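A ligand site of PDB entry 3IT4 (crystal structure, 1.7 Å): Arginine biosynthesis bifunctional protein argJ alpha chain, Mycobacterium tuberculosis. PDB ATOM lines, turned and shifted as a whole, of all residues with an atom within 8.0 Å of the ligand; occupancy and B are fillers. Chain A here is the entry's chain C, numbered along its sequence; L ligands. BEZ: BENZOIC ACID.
NH1 of Arg 9 is in salt-bridge range of O2 of the ligand (2.9 Å).
The side-chain amide nitrogen (NE2) of Gln 14 sits at hydrogen-bond distance from an oxygen (O2) of the ligand, 3.1 Å away.
Residues that only touch the ligand: His 177 (3.5 Å) and Leu 154 (3.7 Å).
Hydrophobic or aromatic side chains within 4 Å of the ligand: Leu 154 and His 177.
Within 4 Å of the ligand: Arg 9, Gln 14, Leu 154 and His 177.
The backbone carbonyl oxygen (O) of Arg 9 sits at hydrogen-bond distance from the backbone NH (N) of His 177 (2.7 Å).
OE1 of Gln 14 sits at hydrogen-bond distance from NE2 of His 177, 2.8 Å away.
O of Gln 14 sits at hydrogen-bond distance from N of Ala 175.
ND1 of His 177 lies within hydrogen-bond range of OG1 of Thr 183, at 3.0 Å.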
ATOM      1  N   ARG A   9      11.513  20.612  -4.871  1.00  0.00           N
ATOM      2  CA  ARG A   9      12.461  20.578  -5.987  1.00  0.00           C
ATOM      3  C   ARG A   9      12.572  21.998  -6.538  1.00  0.00           C
ATOM      4  O   ARG A   9      11.545  22.589  -6.902  1.00  0.00           O
ATOM      5  CB  ARG A   9      11.955  19.656  -7.115  1.00  0.00           C
ATOM      6  CG  ARG A   9      11.788  18.122  -6.789  1.00  0.00           C
ATOM      7  CD  ARG A   9      11.048  17.326  -7.949  1.00  0.00           C
ATOM      8  NE  ARG A   9       9.640  17.723  -8.113  1.00  0.00           N
ATOM      9  CZ  ARG A   9       9.087  18.087  -9.257  1.00  0.00           C
ATOM     10  NH1 ARG A   9       9.778  18.072 -10.396  1.00  0.00           N
ATOM     11  NH2 ARG A   9       7.810  18.461  -9.311  1.00  0.00           N
ATOM     12  N   LEU A  11      14.057  23.705  -9.750  1.00  0.00           N
ATOM     13  CA  LEU A  11      14.485  23.239 -11.085  1.00  0.00           C
ATOM     14  C   LEU A  11      14.565  24.364 -12.079  1.00  0.00           C
ATOM     15  O   LEU A  11      13.604  25.149 -12.234  1.00  0.00           O
ATOM     16  CB  LEU A  11      13.498  22.182 -11.608  1.00  0.00           C
ATOM     17  CG  LEU A  11      13.487  20.848 -10.848  1.00  0.00           C
ATOM     18  CD1 LEU A  11      12.275  19.981 -11.248  1.00  0.00           C
ATOM     19  CD2 LEU A  11      14.780  20.122 -11.096  1.00  0.00           C
ATOM     20  N   ARG A  12      15.684  24.438 -12.767  1.00  0.00           N
ATOM     21  CA  ARG A  12      15.852  25.310 -13.930  1.00  0.00           C
ATOM     22  C   ARG A  12      15.107  24.710 -15.120  1.00  0.00           C
ATOM     23  O   ARG A  12      14.501  23.631 -14.993  1.00  0.00           O
ATOM     24  CB  ARG A  12      17.340  25.510 -14.239  1.00  0.00           C
ATOM     25  CG  ARG A  12      17.975  26.401 -13.177  1.00  0.00           C
ATOM     26  CD  ARG A  12      19.386  26.762 -13.520  1.00  0.00           C
ATOM     27  NE  ARG A  12      19.984  27.531 -12.442  1.00  0.00           N
ATOM     28  CZ  ARG A  12      21.243  27.943 -12.408  1.00  0.00           C
ATOM     29  NH1 ARG A  12      22.084  27.699 -13.421  1.00  0.00           N
ATOM     30  NH2 ARG A  12      21.673  28.621 -11.347  1.00  0.00           N
ATOM     31  N   ALA A  13      15.075  25.438 -16.235  1.00  0.00           N
ATOM     32  CA  ALA A  13      14.348  25.030 -17.454  1.00  0.00           C
ATOM     33  C   ALA A  13      12.833  24.917 -17.252  1.00  0.00           C
ATOM     34  O   ALA A  13      12.132  24.259 -18.032  1.00  0.00           O
ATOM     35  CB  ALA A  13      14.915  23.734 -18.065  1.00  0.00           C
ATOM     36  N   GLN A  14      12.313  25.567 -16.220  1.00  0.00           N
ATOM     37  CA  GLN A  14      10.863  25.717 -16.043  1.00  0.00           C
ATOM     38  C   GLN A  14      10.623  27.131 -15.567  1.00  0.00           C
ATOM     39  O   GLN A  14      11.485  27.656 -14.861  1.00  0.00           O
ATOM     40  CB  GLN A  14      10.364  24.750 -14.964  1.00  0.00           C
ATOM     41  CG  GLN A  14      10.427  23.326 -15.365  1.00  0.00           C
ATOM     42  CD  GLN A  14       9.815  22.450 -14.313  1.00  0.00           C
ATOM     43  OE1 GLN A  14       8.750  22.764 -13.769  1.00  0.00           O
ATOM     44  NE2 GLN A  14      10.470  21.334 -14.014  1.00  0.00           N
ATOM     45  N   ALA A  18       5.010  27.000 -15.024  1.00  0.00           N
ATOM     46  CA  ALA A  18       5.065  25.830 -14.111  1.00  0.00           C
ATOM     47  C   ALA A  18       3.884  25.739 -13.103  1.00  0.00           C
ATOM     48  O   ALA A  18       3.263  24.646 -12.968  1.00  0.00           O
ATOM     49  CB  ALA A  18       6.428  25.758 -13.404  1.00  0.00           C
ATOM     50  N   LEU A 154       4.849  24.375 -20.744  1.00  0.00           N
ATOM     51  CA  LEU A 154       6.183  24.910 -20.430  1.00  0.00           C
ATOM     52  C   LEU A 154       6.855  25.688 -21.553  1.00  0.00           C
ATOM     53  O   LEU A 154       7.618  26.617 -21.286  1.00  0.00           O
ATOM     54  CB  LEU A 154       7.110  23.805 -19.903  1.00  0.00           C
ATOM     55  CG  LEU A 154       6.724  23.243 -18.526  1.00  0.00           C
ATOM     56  CD1 LEU A 154       7.600  22.011 -18.181  1.00  0.00           C
ATOM     57  CD2 LEU A 154       6.831  24.316 -17.468  1.00  0.00           C
ATOM     58  N   ALA A 175      11.810  27.166 -11.434  1.00  0.00           N
ATOM     59  CA  ALA A 175      10.604  26.935 -10.713  1.00  0.00           C
ATOM     60  C   ALA A 175      10.881  26.169  -9.433  1.00  0.00           C
ATOM     61  O   ALA A 175      11.736  25.264  -9.416  1.00  0.00           O
ATOM     62  CB  ALA A 175       9.515  26.187 -11.604  1.00  0.00           C
ATOM     63  N   HIS A 177       9.079  23.662  -6.887  1.00  0.00           N
ATOM     64  CA  HIS A 177       7.937  22.769  -6.630  1.00  0.00           C
ATOM     65  C   HIS A 177       7.958  22.380  -5.142  1.00  0.00           C
ATOM     66  O   HIS A 177       8.846  21.656  -4.703  1.00  0.00           O
ATOM     67  CB  HIS A 177       7.971  21.517  -7.541  1.00  0.00           C
ATOM     68  CG  HIS A 177       7.786  21.833  -8.989  1.00  0.00           C
ATOM     69  ND1 HIS A 177       6.538  21.998  -9.573  1.00  0.00           N
ATOM     70  CD2 HIS A 177       8.690  22.018  -9.986  1.00  0.00           C
ATOM     71  CE1 HIS A 177       6.687  22.273 -10.851  1.00  0.00           C
ATOM     72  NE2 HIS A 177       7.978  22.295 -11.133  1.00  0.00           N
ATOM     73  N   THR A 183       3.528  25.717  -6.284  1.00  0.00           N
ATOM     74  CA  THR A 183       4.737  25.965  -7.061  1.00  0.00           C
ATOM     75  C   THR A 183       4.929  27.471  -7.253  1.00  0.00           C
ATOM     76  O   THR A 183       3.947  28.178  -7.415  1.00  0.00           O
ATOM     77  CB  THR A 183       4.602  25.285  -8.439  1.00  0.00           C
ATOM     78  OG1 THR A 183       4.641  23.873  -8.267  1.00  0.00           O
ATOM     79  CG2 THR A 183       5.722  25.688  -9.392  1.00  0.00           C
HETATM   80  C   BEZ L   1       7.455  18.824 -12.998  1.00  0.00           C
HETATM   81  O1  BEZ L   1       6.675  18.651 -12.026  1.00  0.00           O
HETATM   82  O2  BEZ L   1       8.618  19.244 -12.764  1.00  0.00           O
HETATM   83  C1  BEZ L   1       6.986  18.513 -14.415  1.00  0.00           C
HETATM   84  C2  BEZ L   1       5.740  17.876 -14.617  1.00  0.00           C
HETATM   85  C3  BEZ L   1       5.301  17.577 -15.907  1.00  0.00           C
HETATM   86  C4  BEZ L   1       6.104  17.928 -17.009  1.00  0.00           C
HETATM   87  C5  BEZ L   1       7.341  18.561 -16.820  1.00  0.00           C
HETATM   88  C6  BEZ L   1       7.785  18.847 -15.516  1.00  0.00           C
